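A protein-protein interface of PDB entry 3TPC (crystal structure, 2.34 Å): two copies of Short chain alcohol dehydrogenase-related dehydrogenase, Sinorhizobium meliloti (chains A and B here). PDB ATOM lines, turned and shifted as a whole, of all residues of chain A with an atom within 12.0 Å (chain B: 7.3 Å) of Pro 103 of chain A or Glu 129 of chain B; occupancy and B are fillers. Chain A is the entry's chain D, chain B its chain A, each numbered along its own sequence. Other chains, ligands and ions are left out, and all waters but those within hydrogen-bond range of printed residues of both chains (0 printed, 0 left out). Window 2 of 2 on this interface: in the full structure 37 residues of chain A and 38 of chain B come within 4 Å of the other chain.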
ATOM      1  N   GLY A  94      -5.706 -12.814  10.988  1.00  0.00           N
ATOM      2  CA  GLY A  94      -4.950 -13.977  11.434  1.00  0.00           C
ATOM      3  C   GLY A  94      -5.323 -14.136  12.897  1.00  0.00           C
ATOM      4  O   GLY A  94      -5.356 -13.162  13.643  1.00  0.00           O
ATOM      5  N   GLU A  95      -5.654 -15.362  13.283  1.00  0.00           N
ATOM      6  CA  GLU A  95      -5.990 -15.726  14.634  1.00  0.00           C
ATOM      7  C   GLU A  95      -5.729 -17.225  14.678  1.00  0.00           C
ATOM      8  O   GLU A  95      -6.135 -17.969  13.763  1.00  0.00           O
ATOM      9  CB  GLU A  95      -7.477 -15.450  14.869  1.00  0.00           C
ATOM     10  CG  GLU A  95      -7.897 -15.280  16.345  1.00  0.00           C
ATOM     11  CD  GLU A  95      -9.383 -14.887  16.549  1.00  0.00           C
ATOM     12  OE1 GLU A  95      -9.977 -14.213  15.673  1.00  0.00           O
ATOM     13  OE2 GLU A  95      -9.950 -15.242  17.616  1.00  0.00           O
ATOM     14  N   LYS A  96      -5.043 -17.691  15.716  1.00  0.00           N
ATOM     15  CA  LYS A  96      -4.837 -19.131  15.823  1.00  0.00           C
ATOM     16  C   LYS A  96      -6.104 -19.858  16.244  1.00  0.00           C
ATOM     17  O   LYS A  96      -6.962 -19.317  16.932  1.00  0.00           O
ATOM     18  CB  LYS A  96      -3.697 -19.466  16.769  1.00  0.00           C
ATOM     19  CG  LYS A  96      -2.361 -18.874  16.344  1.00  0.00           C
ATOM     20  CD  LYS A  96      -1.289 -19.058  17.401  1.00  0.00           C
ATOM     21  CE  LYS A  96       0.069 -18.961  16.732  1.00  0.00           C
ATOM     22  NZ  LYS A  96       1.189 -19.071  17.719  1.00  0.00           N
ATOM     23  N   ILE A  97      -6.223 -21.100  15.792  1.00  0.00           N
ATOM     24  CA  ILE A  97      -7.259 -21.963  16.270  1.00  0.00           C
ATOM     25  C   ILE A  97      -7.169 -22.045  17.784  1.00  0.00           C
ATOM     26  O   ILE A  97      -8.169 -21.855  18.442  1.00  0.00           O
ATOM     27  CB  ILE A  97      -7.165 -23.391  15.661  1.00  0.00           C
ATOM     28  CG1 ILE A  97      -7.247 -23.322  14.121  1.00  0.00           C
ATOM     29  CG2 ILE A  97      -8.222 -24.325  16.292  1.00  0.00           C
ATOM     30  CD1 ILE A  97      -6.972 -24.646  13.429  1.00  0.00           C
ATOM     31  N   LEU A  98      -5.982 -22.358  18.325  1.00  0.00           N
ATOM     32  CA  LEU A  98      -5.826 -22.541  19.783  1.00  0.00           C
ATOM     33  C   LEU A  98      -4.852 -21.504  20.235  1.00  0.00           C
ATOM     34  O   LEU A  98      -3.674 -21.712  20.143  1.00  0.00           O
ATOM     35  CB  LEU A  98      -5.297 -23.955  20.149  1.00  0.00           C
ATOM     36  CG  LEU A  98      -6.197 -25.165  20.033  1.00  0.00           C
ATOM     37  CD1 LEU A  98      -5.535 -26.371  20.650  1.00  0.00           C
ATOM     38  CD2 LEU A  98      -7.583 -24.963  20.665  1.00  0.00           C
ATOM     39  N   GLY A  99      -5.351 -20.363  20.677  1.00  0.00           N
ATOM     40  CA  GLY A  99      -4.466 -19.248  21.090  1.00  0.00           C
ATOM     41  C   GLY A  99      -4.058 -19.237  22.566  1.00  0.00           C
ATOM     42  O   GLY A  99      -4.607 -20.004  23.380  1.00  0.00           O
ATOM     43  N   ARG A 100      -3.096 -18.378  22.916  1.00  0.00           N
ATOM     44  CA  ARG A 100      -2.661 -18.224  24.323  1.00  0.00           C
ATOM     45  C   ARG A 100      -3.894 -18.020  25.239  1.00  0.00           C
ATOM     46  O   ARG A 100      -4.043 -18.674  26.269  1.00  0.00           O
ATOM     47  CB  ARG A 100      -1.669 -17.060  24.450  1.00  0.00           C
ATOM     48  N   SER A 101      -4.803 -17.153  24.808  1.00  0.00           N
ATOM     49  CA  SER A 101      -6.021 -16.814  25.560  1.00  0.00           C
ATOM     50  C   SER A 101      -7.077 -17.926  25.639  1.00  0.00           C
ATOM     51  O   SER A 101      -7.673 -18.164  26.710  1.00  0.00           O
ATOM     52  CB  SER A 101      -6.672 -15.609  24.888  1.00  0.00           C
ATOM     53  OG  SER A 101      -8.068 -15.638  25.123  1.00  0.00           O
ATOM     54  N   GLY A 102      -7.333 -18.563  24.498  1.00  0.00           N
ATOM     55  CA  GLY A 102      -8.307 -19.644  24.386  1.00  0.00           C
ATOM     56  C   GLY A 102      -8.501 -19.954  22.908  1.00  0.00           C
ATOM     57  O   GLY A 102      -7.796 -19.423  22.057  1.00  0.00           O
ATOM     58  N   PRO A 103      -9.456 -20.815  22.583  1.00  0.00           N
ATOM     59  CA  PRO A 103      -9.741 -21.053  21.157  1.00  0.00           C
ATOM     60  C   PRO A 103     -10.208 -19.818  20.391  1.00  0.00           C
ATOM     61  O   PRO A 103     -10.726 -18.853  20.978  1.00  0.00           O
ATOM     62  CB  PRO A 103     -10.840 -22.138  21.166  1.00  0.00           C
ATOM     63  CG  PRO A 103     -11.282 -22.254  22.581  1.00  0.00           C
ATOM     64  CD  PRO A 103     -10.221 -21.693  23.484  1.00  0.00           C
ATOM     65  N   HIS A 104     -10.004 -19.867  19.085  1.00  0.00           N
ATOM     66  CA  HIS A 104     -10.364 -18.855  18.133  1.00  0.00           C
ATOM     67  C   HIS A 104     -11.821 -18.498  18.375  1.00  0.00           C
ATOM     68  O   HIS A 104     -12.621 -19.381  18.498  1.00  0.00           O
ATOM     69  CB  HIS A 104     -10.214 -19.556  16.798  1.00  0.00           C
ATOM     70  CG  HIS A 104     -10.264 -18.672  15.604  1.00  0.00           C
ATOM     71  ND1 HIS A 104     -11.384 -17.949  15.257  1.00  0.00           N
ATOM     72  CD2 HIS A 104      -9.354 -18.461  14.620  1.00  0.00           C
ATOM     73  CE1 HIS A 104     -11.142 -17.275  14.145  1.00  0.00           C
ATOM     74  NE2 HIS A 104      -9.918 -17.573  13.734  1.00  0.00           N
ATOM     75  N   ALA A 105     -12.185 -17.215  18.464  1.00  0.00           N
ATOM     76  CA  ALA A 105     -13.592 -16.857  18.692  1.00  0.00           C
ATOM     77  C   ALA A 105     -14.457 -17.438  17.562  1.00  0.00           C
ATOM     78  O   ALA A 105     -14.055 -17.395  16.375  1.00  0.00           O
ATOM     79  CB  ALA A 105     -13.739 -15.365  18.715  1.00  0.00           C
ATOM     80  N   LEU A 106     -15.633 -17.948  17.899  1.00  0.00           N
ATOM     81  CA  LEU A 106     -16.540 -18.401  16.867  1.00  0.00           C
ATOM     82  C   LEU A 106     -16.972 -17.313  15.881  1.00  0.00           C
ATOM     83  O   LEU A 106     -16.804 -17.439  14.655  1.00  0.00           O
ATOM     84  CB  LEU A 106     -17.792 -19.058  17.459  1.00  0.00           C
ATOM     85  CG  LEU A 106     -18.543 -19.823  16.362  1.00  0.00           C
ATOM     86  CD1 LEU A 106     -17.530 -20.749  15.612  1.00  0.00           C
ATOM     87  CD2 LEU A 106     -19.753 -20.613  16.889  1.00  0.00           C
ATOM     88  N   ASP A 107     -17.555 -16.264  16.410  1.00  0.00           N
ATOM     89  CA  ASP A 107     -18.170 -15.222  15.602  1.00  0.00           C
ATOM     90  C   ASP A 107     -17.168 -14.469  14.731  1.00  0.00           C
ATOM     91  O   ASP A 107     -17.529 -13.975  13.687  1.00  0.00           O
ATOM     92  CB  ASP A 107     -18.917 -14.233  16.502  1.00  0.00           C
ATOM     93  CG  ASP A 107     -18.063 -13.003  16.847  1.00  0.00           C
ATOM     94  OD1 ASP A 107     -17.944 -12.063  15.989  1.00  0.00           O
ATOM     95  OD2 ASP A 107     -17.481 -12.974  17.950  1.00  0.00           O
ATOM     96  N   SER A 108     -15.927 -14.346  15.181  1.00  0.00           N
ATOM     97  CA  SER A 108     -14.846 -13.802  14.362  1.00  0.00           C
ATOM     98  C   SER A 108     -14.662 -14.583  13.019  1.00  0.00           C
ATOM     99  O   SER A 108     -14.525 -13.980  11.934  1.00  0.00           O
ATOM    100  CB  SER A 108     -13.561 -13.826  15.159  1.00  0.00           C
ATOM    101  OG  SER A 108     -12.531 -13.311  14.367  1.00  0.00           O
ATOM    102  N   PHE A 109     -14.687 -15.911  13.123  1.00  0.00           N
ATOM    103  CA  PHE A 109     -14.547 -16.841  12.001  1.00  0.00           C
ATOM    104  C   PHE A 109     -15.733 -16.731  11.005  1.00  0.00           C
ATOM    105  O   PHE A 109     -15.533 -16.549   9.785  1.00  0.00           O
ATOM    106  CB  PHE A 109     -14.396 -18.275  12.542  1.00  0.00           C
ATOM    107  CG  PHE A 109     -14.282 -19.289  11.490  1.00  0.00           C
ATOM    108  CD1 PHE A 109     -13.037 -19.734  11.080  1.00  0.00           C
ATOM    109  CD2 PHE A 109     -15.439 -19.801  10.864  1.00  0.00           C
ATOM    110  CE1 PHE A 109     -12.920 -20.664  10.040  1.00  0.00           C
ATOM    111  CE2 PHE A 109     -15.341 -20.751   9.842  1.00  0.00           C
ATOM    112  CZ  PHE A 109     -14.089 -21.159   9.419  1.00  0.00           C
ATOM    113  N   ALA A 110     -16.947 -16.793  11.559  1.00  0.00           N
ATOM    114  CA  ALA A 110     -18.192 -16.478  10.848  1.00  0.00           C
ATOM    115  C   ALA A 110     -18.144 -15.147  10.122  1.00  0.00           C
ATOM    116  O   ALA A 110     -18.516 -15.054   8.973  1.00  0.00           O
ATOM    117  CB  ALA A 110     -19.398 -16.545  11.799  1.00  0.00           C
ATOM    118  N   GLY A 159      -2.429 -19.605  11.524  1.00  0.00           N
ATOM    119  CA  GLY A 159      -3.185 -18.417  11.817  1.00  0.00           C
ATOM    120  C   GLY A 159      -4.135 -18.014  10.699  1.00  0.00           C
ATOM    121  O   GLY A 159      -4.907 -17.063  10.843  1.00  0.00           O
ATOM    122  N   ALA A 161      -6.599 -19.897   9.229  1.00  0.00           N
ATOM    123  CA  ALA A 161      -7.726 -20.801   9.055  1.00  0.00           C
ATOM    124  C   ALA A 161      -8.998 -20.200   8.417  1.00  0.00           C
ATOM    125  O   ALA A 161      -9.591 -20.788   7.490  1.00  0.00           O
ATOM    126  CB  ALA A 161      -8.099 -21.459  10.390  1.00  0.00           C
ATOM    127  N   ALA A 162      -9.427 -19.064   8.948  1.00  0.00           N
ATOM    128  CA  ALA A 162     -10.701 -18.439   8.592  1.00  0.00           C
ATOM    129  C   ALA A 162     -10.573 -17.836   7.206  1.00  0.00           C
ATOM    130  O   ALA A 162     -11.487 -17.938   6.369  1.00  0.00           O
ATOM    131  CB  ALA A 162     -11.090 -17.355   9.640  1.00  0.00           C
ATOM    132  N   LEU B  72     -18.637 -30.745  24.669  1.00  0.00           N
ATOM    133  CA  LEU B  72     -17.278 -30.878  25.158  1.00  0.00           C
ATOM    134  C   LEU B  72     -17.257 -31.015  26.679  1.00  0.00           C
ATOM    135  O   LEU B  72     -16.610 -31.899  27.200  1.00  0.00           O
ATOM    136  CB  LEU B  72     -16.383 -29.709  24.700  1.00  0.00           C
ATOM    137  CG  LEU B  72     -15.581 -29.903  23.397  1.00  0.00           C
ATOM    138  CD1 LEU B  72     -14.645 -31.043  23.506  1.00  0.00           C
ATOM    139  CD2 LEU B  72     -16.474 -30.135  22.183  1.00  0.00           C
ATOM    140  N   PHE B 121     -15.740 -26.111  11.888  1.00  0.00           N
ATOM    141  CA  PHE B 121     -14.681 -25.324  12.541  1.00  0.00           C
ATOM    142  C   PHE B 121     -14.886 -25.168  14.064  1.00  0.00           C
ATOM    143  O   PHE B 121     -13.958 -25.235  14.880  1.00  0.00           O
ATOM    144  CB  PHE B 121     -14.450 -23.978  11.841  1.00  0.00           C
ATOM    145  CG  PHE B 121     -13.368 -23.151  12.484  1.00  0.00           C
ATOM    146  CD1 PHE B 121     -12.020 -23.395  12.200  1.00  0.00           C
ATOM    147  CD2 PHE B 121     -13.694 -22.169  13.412  1.00  0.00           C
ATOM    148  CE1 PHE B 121     -11.022 -22.642  12.818  1.00  0.00           C
ATOM    149  CE2 PHE B 121     -12.709 -21.404  14.018  1.00  0.00           C
ATOM    150  CZ  PHE B 121     -11.376 -21.651  13.740  1.00  0.00           C
ATOM    151  N   ASN B 122     -16.126 -24.948  14.429  1.00  0.00           N
ATOM    152  CA  ASN B 122     -16.543 -24.846  15.785  1.00  0.00           C
ATOM    153  C   ASN B 122     -16.191 -26.108  16.575  1.00  0.00           C
ATOM    154  O   ASN B 122     -15.644 -26.009  17.683  1.00  0.00           O
ATOM    155  CB  ASN B 122     -18.050 -24.591  15.773  1.00  0.00           C
ATOM    156  CG  ASN B 122     -18.619 -24.203  17.102  1.00  0.00           C
ATOM    157  OD1 ASN B 122     -19.758 -24.568  17.394  1.00  0.00           O
ATOM    158  ND2 ASN B 122     -17.902 -23.420  17.883  1.00  0.00           N
ATOM    159  N   MET B 123     -16.458 -27.287  16.014  1.00  0.00           N
ATOM    160  CA  MET B 123     -16.098 -28.500  16.698  1.00  0.00           C
ATOM    161  C   MET B 123     -14.567 -28.666  16.764  1.00  0.00           C
ATOM    162  O   MET B 123     -14.046 -29.160  17.757  1.00  0.00           O
ATOM    163  CB  MET B 123     -16.764 -29.728  16.077  1.00  0.00           C
ATOM    164  CG  MET B 123     -18.276 -29.701  16.169  1.00  0.00           C
ATOM    165  SD  MET B 123     -18.822 -29.780  18.047  1.00  0.00           S
ATOM    166  CE  MET B 123     -17.647 -28.510  18.848  1.00  0.00           C
ATOM    167  N   ILE B 124     -13.857 -28.245  15.726  1.00  0.00           N
ATOM    168  CA  ILE B 124     -12.408 -28.309  15.716  1.00  0.00           C
ATOM    169  C   ILE B 124     -11.759 -27.436  16.813  1.00  0.00           C
ATOM    170  O   ILE B 124     -10.955 -27.951  17.573  1.00  0.00           O
ATOM    171  CB  ILE B 124     -11.820 -27.938  14.306  1.00  0.00           C
ATOM    172  CG1 ILE B 124     -11.915 -29.115  13.324  1.00  0.00           C
ATOM    173  CG2 ILE B 124     -10.374 -27.420  14.396  1.00  0.00           C
ATOM    174  CD1 ILE B 124     -11.830 -28.646  11.827  1.00  0.00           C
ATOM    175  N   ARG B 125     -12.096 -26.142  16.884  1.00  0.00           N
ATOM    176  CA  ARG B 125     -11.459 -25.213  17.835  1.00  0.00           C
ATOM    177  C   ARG B 125     -11.588 -25.704  19.264  1.00  0.00           C
ATOM    178  O   ARG B 125     -10.646 -25.574  20.057  1.00  0.00           O
ATOM    179  CB  ARG B 125     -12.074 -23.817  17.746  1.00  0.00           C
ATOM    180  CG  ARG B 125     -13.547 -23.788  18.032  1.00  0.00           C
ATOM    181  CD  ARG B 125     -14.171 -22.492  17.494  1.00  0.00           C
ATOM    182  NE  ARG B 125     -14.132 -21.507  18.549  1.00  0.00           N
ATOM    183  CZ  ARG B 125     -15.056 -21.336  19.487  1.00  0.00           C
ATOM    184  NH1 ARG B 125     -16.176 -22.059  19.510  1.00  0.00           N
ATOM    185  NH2 ARG B 125     -14.831 -20.426  20.417  1.00  0.00           N
ATOM    186  N   LEU B 126     -12.741 -26.289  19.584  1.00  0.00           N
ATOM    187  CA  LEU B 126     -13.039 -26.772  20.929  1.00  0.00           C
ATOM    188  C   LEU B 126     -12.561 -28.209  21.209  1.00  0.00           C
ATOM    189  O   LEU B 126     -12.074 -28.475  22.293  1.00  0.00           O
ATOM    190  CB  LEU B 126     -14.537 -26.666  21.222  1.00  0.00           C
ATOM    191  CG  LEU B 126     -15.147 -25.257  21.247  1.00  0.00           C
ATOM    192  CD1 LEU B 126     -16.617 -25.402  21.551  1.00  0.00           C
ATOM    193  CD2 LEU B 126     -14.496 -24.321  22.301  1.00  0.00           C
ATOM    194  N   ALA B 127     -12.766 -29.143  20.281  1.00  0.00           N
ATOM    195  CA  ALA B 127     -12.219 -30.506  20.460  1.00  0.00           C
ATOM    196  C   ALA B 127     -10.701 -30.456  20.649  1.00  0.00           C
ATOM    197  O   ALA B 127     -10.154 -31.142  21.523  1.00  0.00           O
ATOM    198  CB  ALA B 127     -12.569 -31.415  19.316  1.00  0.00           C
ATOM    199  N   ALA B 128     -10.055 -29.595  19.865  1.00  0.00           N
ATOM    200  CA  ALA B 128      -8.600 -29.480  19.815  1.00  0.00           C
ATOM    201  C   ALA B 128      -8.050 -28.965  21.116  1.00  0.00           C
ATOM    202  O   ALA B 128      -6.980 -29.403  21.532  1.00  0.00           O
ATOM    203  CB  ALA B 128      -8.163 -28.552  18.655  1.00  0.00           C
ATOM    204  N   GLU B 129      -8.797 -28.102  21.786  1.00  0.00           N
ATOM    205  CA  GLU B 129      -8.356 -27.533  23.025  1.00  0.00           C
ATOM    206  C   GLU B 129      -8.146 -28.659  24.017  1.00  0.00           C
ATOM    207  O   GLU B 129      -7.172 -28.697  24.695  1.00  0.00           O
ATOM    208  CB  GLU B 129      -9.418 -26.532  23.530  1.00  0.00           C
ATOM    209  CG  GLU B 129      -9.023 -25.569  24.651  1.00  0.00           C
ATOM    210  CD  GLU B 129     -10.181 -24.768  25.295  1.00  0.00           C
ATOM    211  OE1 GLU B 129     -11.360 -24.984  25.027  1.00  0.00           O
ATOM    212  OE2 GLU B 129      -9.918 -23.882  26.111  1.00  0.00           O
ATOM    213  N   VAL B 130      -9.098 -29.564  24.076  1.00  0.00           N
ATOM    214  CA  VAL B 130      -9.011 -30.779  24.850  1.00  0.00           C
ATOM    215  C   VAL B 130      -8.005 -31.873  24.490  1.00  0.00           C
ATOM    216  O   VAL B 130      -7.417 -32.444  25.351  1.00  0.00           O
ATOM    217  CB  VAL B 130     -10.360 -31.339  25.076  1.00  0.00           C
ATOM    218  CG1 VAL B 130     -10.271 -32.525  25.849  1.00  0.00           C
ATOM    219  CG2 VAL B 130     -11.147 -30.368  25.787  1.00  0.00           C
ATOM    220  N   MET B 131      -7.826 -32.158  23.220  1.00  0.00           N
ATOM    221  CA  MET B 131      -6.896 -33.166  22.775  1.00  0.00           C
ATOM    222  C   MET B 131      -5.514 -32.747  23.172  1.00  0.00           C
ATOM    223  O   MET B 131      -4.704 -33.525  23.503  1.00  0.00           O
ATOM    224  CB  MET B 131      -6.955 -33.360  21.276  1.00  0.00           C
ATOM    225  CG  MET B 131      -8.327 -33.421  20.645  1.00  0.00           C
ATOM    226  SD  MET B 131      -8.422 -33.944  18.810  1.00  0.00           S
ATOM    227  CE  MET B 131     -10.130 -34.426  18.814  1.00  0.00           C
ATOM    228  N   SER B 132      -5.310 -31.463  23.101  1.00  0.00           N
ATOM    229  CA  SER B 132      -4.125 -30.728  23.393  1.00  0.00           C
ATOM    230  C   SER B 132      -3.551 -31.048  24.763  1.00  0.00           C
ATOM    231  O   SER B 132      -2.377 -31.039  24.959  1.00  0.00           O
ATOM    232  CB  SER B 132      -4.639 -29.307  23.512  1.00  0.00           C
ATOM    233  OG  SER B 132      -3.724 -28.338  23.179  1.00  0.00           O
ATOM    234  N   GLN B 133      -4.428 -31.254  25.710  1.00  0.00           N
ATOM    235  CA  GLN B 133      -4.096 -31.543  27.101  1.00  0.00           C
ATOM    236  C   GLN B 133      -3.831 -33.038  27.431  1.00  0.00           C
ATOM    237  O   GLN B 133      -3.392 -33.355  28.531  1.00  0.00           O
ATOM    238  CB  GLN B 133      -5.214 -30.991  27.984  1.00  0.00           C
ATOM    239  CG  GLN B 133      -5.546 -29.474  27.717  1.00  0.00           C
ATOM    240  CD  GLN B 133      -4.271 -28.564  27.690  1.00  0.00           C
ATOM    241  OE1 GLN B 133      -4.161 -27.634  26.859  1.00  0.00           O
ATOM    242  NE2 GLN B 133      -3.309 -28.844  28.590  1.00  0.00           N
ATOM    243  N   GLY B 134      -4.061 -33.940  26.484  1.00  0.00           N
ATOM    244  CA  GLY B 134      -3.939 -35.357  26.776  1.00  0.00           C
ATOM    245  C   GLY B 134      -2.523 -35.887  26.653  1.00  0.00           C
ATOM    246  O   GLY B 134      -1.599 -35.134  26.323  1.00  0.00           O
ATOM    247  N   LEU B 181      -1.792 -27.346  14.426  1.00  0.00           N
ATOM    248  CA  LEU B 181      -2.026 -28.289  15.467  1.00  0.00           C
ATOM    249  C   LEU B 181      -0.962 -29.345  15.538  1.00  0.00           C
ATOM    250  O   LEU B 181      -0.963 -30.138  16.407  1.00  0.00           O
ATOM    251  CB  LEU B 181      -3.392 -28.885  15.340  1.00  0.00           C
ATOM    252  CG  LEU B 181      -4.440 -27.823  15.520  1.00  0.00           C
ATOM    253  CD1 LEU B 181      -5.738 -28.275  15.053  1.00  0.00           C
ATOM    254  CD2 LEU B 181      -4.539 -27.195  16.862  1.00  0.00           C
ATOM    255  N   PHE B 184       0.890 -29.665  18.811  1.00  0.00           N
ATOM    256  CA  PHE B 184       0.382 -30.496  19.886  1.00  0.00           C
ATOM    257  C   PHE B 184       0.299 -31.927  19.475  1.00  0.00           C
ATOM    258  O   PHE B 184      -0.284 -32.727  20.185  1.00  0.00           O
ATOM    259  CB  PHE B 184      -1.014 -30.020  20.293  1.00  0.00           C
ATOM    260  CG  PHE B 184      -1.067 -28.582  20.586  1.00  0.00           C
ATOM    261  CD1 PHE B 184      -0.644 -28.104  21.826  1.00  0.00           C
ATOM    262  CD2 PHE B 184      -1.474 -27.696  19.621  1.00  0.00           C
ATOM    263  CE1 PHE B 184      -0.660 -26.725  22.112  1.00  0.00           C
ATOM    264  CE2 PHE B 184      -1.484 -26.297  19.875  1.00  0.00           C
ATOM    265  CZ  PHE B 184      -1.080 -25.821  21.136  1.00  0.00           C
ATOM    266  N   ILE B 186      -1.583 -33.002  16.990  1.00  0.00           N
ATOM    267  CA  ILE B 186      -2.935 -33.304  16.449  1.00  0.00           C
ATOM    268  C   ILE B 186      -2.999 -33.293  14.885  1.00  0.00           C
ATOM    269  O   ILE B 186      -2.722 -32.288  14.249  1.00  0.00           O
ATOM    270  CB  ILE B 186      -3.957 -32.367  17.024  1.00  0.00           C
ATOM    271  CG1 ILE B 186      -4.074 -32.585  18.536  1.00  0.00           C
ATOM    272  CG2 ILE B 186      -5.269 -32.480  16.330  1.00  0.00           C
ATOM    273  CD1 ILE B 186      -4.666 -31.367  19.234  1.00  0.00           C
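Of chain B, only Arg 125, Leu 126 and Glu 129 come within 4 Å of Pro 103 of chain A. Of the printed residues of chain A, Glu 129 of chain B touches Leu 98 (3.5 Å) and Pro 103 (3.4 Å). Printed residues of chain A within 4 Å of Arg 125 of chain B: Ile 97 (3.7 Å), Leu 98 (3.2 Å), Pro 103 (3.6 Å), His 104 (2.6 Å) and Leu 106 (3.6 Å). Of chain A, only Pro 103 comes within 4 Å of Leu 126 of chain B. No residue of chain A comes within 4 Å of Ala 127 of chain B. Ala 128 of chain B touches one residue of chain A. Val 130 of chain B touches none of the printed residues of chain A. No residue of chain A comes within 4 Å of Met 131 of chain B. Printed residues of chain A within 4 Å of Ser 132 of chain B: Leu 98 (3.7 Å). Of the printed residues of chain B, His 104 of chain A touches Phe 121 (3.7 Å) and Arg 125 (2.6 Å). Of the printed residues of chain B, Ile 97 of chain A touches Arg 125 (3.7 Å). Printed residues of chain A within 4 Å of Asn 122 of chain B: Leu 106 (3.5 Å). Of the printed residues of chain B, Leu 106 of chain A touches Asn 122 (3.5 Å) and Arg 125 (3.6 Å). Phe 184 of chain B touches none of the printed residues of chain A. The nearest residue of chain B that does not touch Pro 103 of chain A is Ile 124 of chain B (6.8 Å). The nearest residue of chain A that does not touch Glu 129 of chain B is Gly 102 of chain A (4.9 Å). The nearest printed residue of chain B that does not touch Ile 97 of chain A is Phe 121 of chain B (4.1 Å).
No position is printed for both chains. Of the 14 pairs that touch across the chains among the printed residues, none has its exchanged pair printed and touching as well.
O of His 104 of chain A sits at hydrogen-bond distance from NE of Arg 125 of chain B.
Of the 20 printed residues of chain A, 7 touch a printed residue of chain B. Hydrophobic or aromatic side chains of chain A within 4 Å of the printed part of chain B: Ile 97, Leu 98, Pro 103, His 104, Leu 106, Phe 109 and Ala 161. Printed residues of chain B that touch a printed residue of chain A: Phe 121, Asn 122, Arg 125, Leu 126, Ala 128, Glu 129 and Ser 132. Hydrophobic or aromatic side chains of chain B within 4 Å of the printed part of chain A: Phe 121, Leu 126 and Ala 128. Among the printed residues, 14 pairs touch across the chains. Among the printed residues, no Asp or Glu carboxylate lies within 4 Å of a Lys or Arg side-chain nitrogen of the other chain.
Among the printed residues, merely in contact across the chains: Leu 98 of chain A with Arg 125 of chain B, Phe 109 of chain A with Phe 121 of chain B, Pro 103 of chain A with Glu 129 of chain B, Leu 98 of chain A with Ala 128 of chain B, Leu 106 of chain A with Asn 122 of chain B, Leu 98 of chain A with Glu 129 of chain B, Pro 103 of chain A with Arg 125 of chain B, Leu 106 of chain A with Arg 125 of chain B, Leu 98 of chain A with Ser 132 of chain B, His 104 of chain A with Phe 121 of chain B, Ile 97 of chain A with Arg 125 of chain B, Pro 103 of chain A with Leu 126 of chain B and Ala 161 of chain A with Phe 121 of chain B.
The side-chain amide nitrogen (ND2) of Asn 122 of chain B sits close to the guanidinium group (NH1) of Arg 125 of chain B, 2.7 Å away. The backbone carbonyl oxygen (O) of Ile 97 of chain A is in hydrogen-bond range of the backbone NH (N) of His 104 of chain A (2.8 Å).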
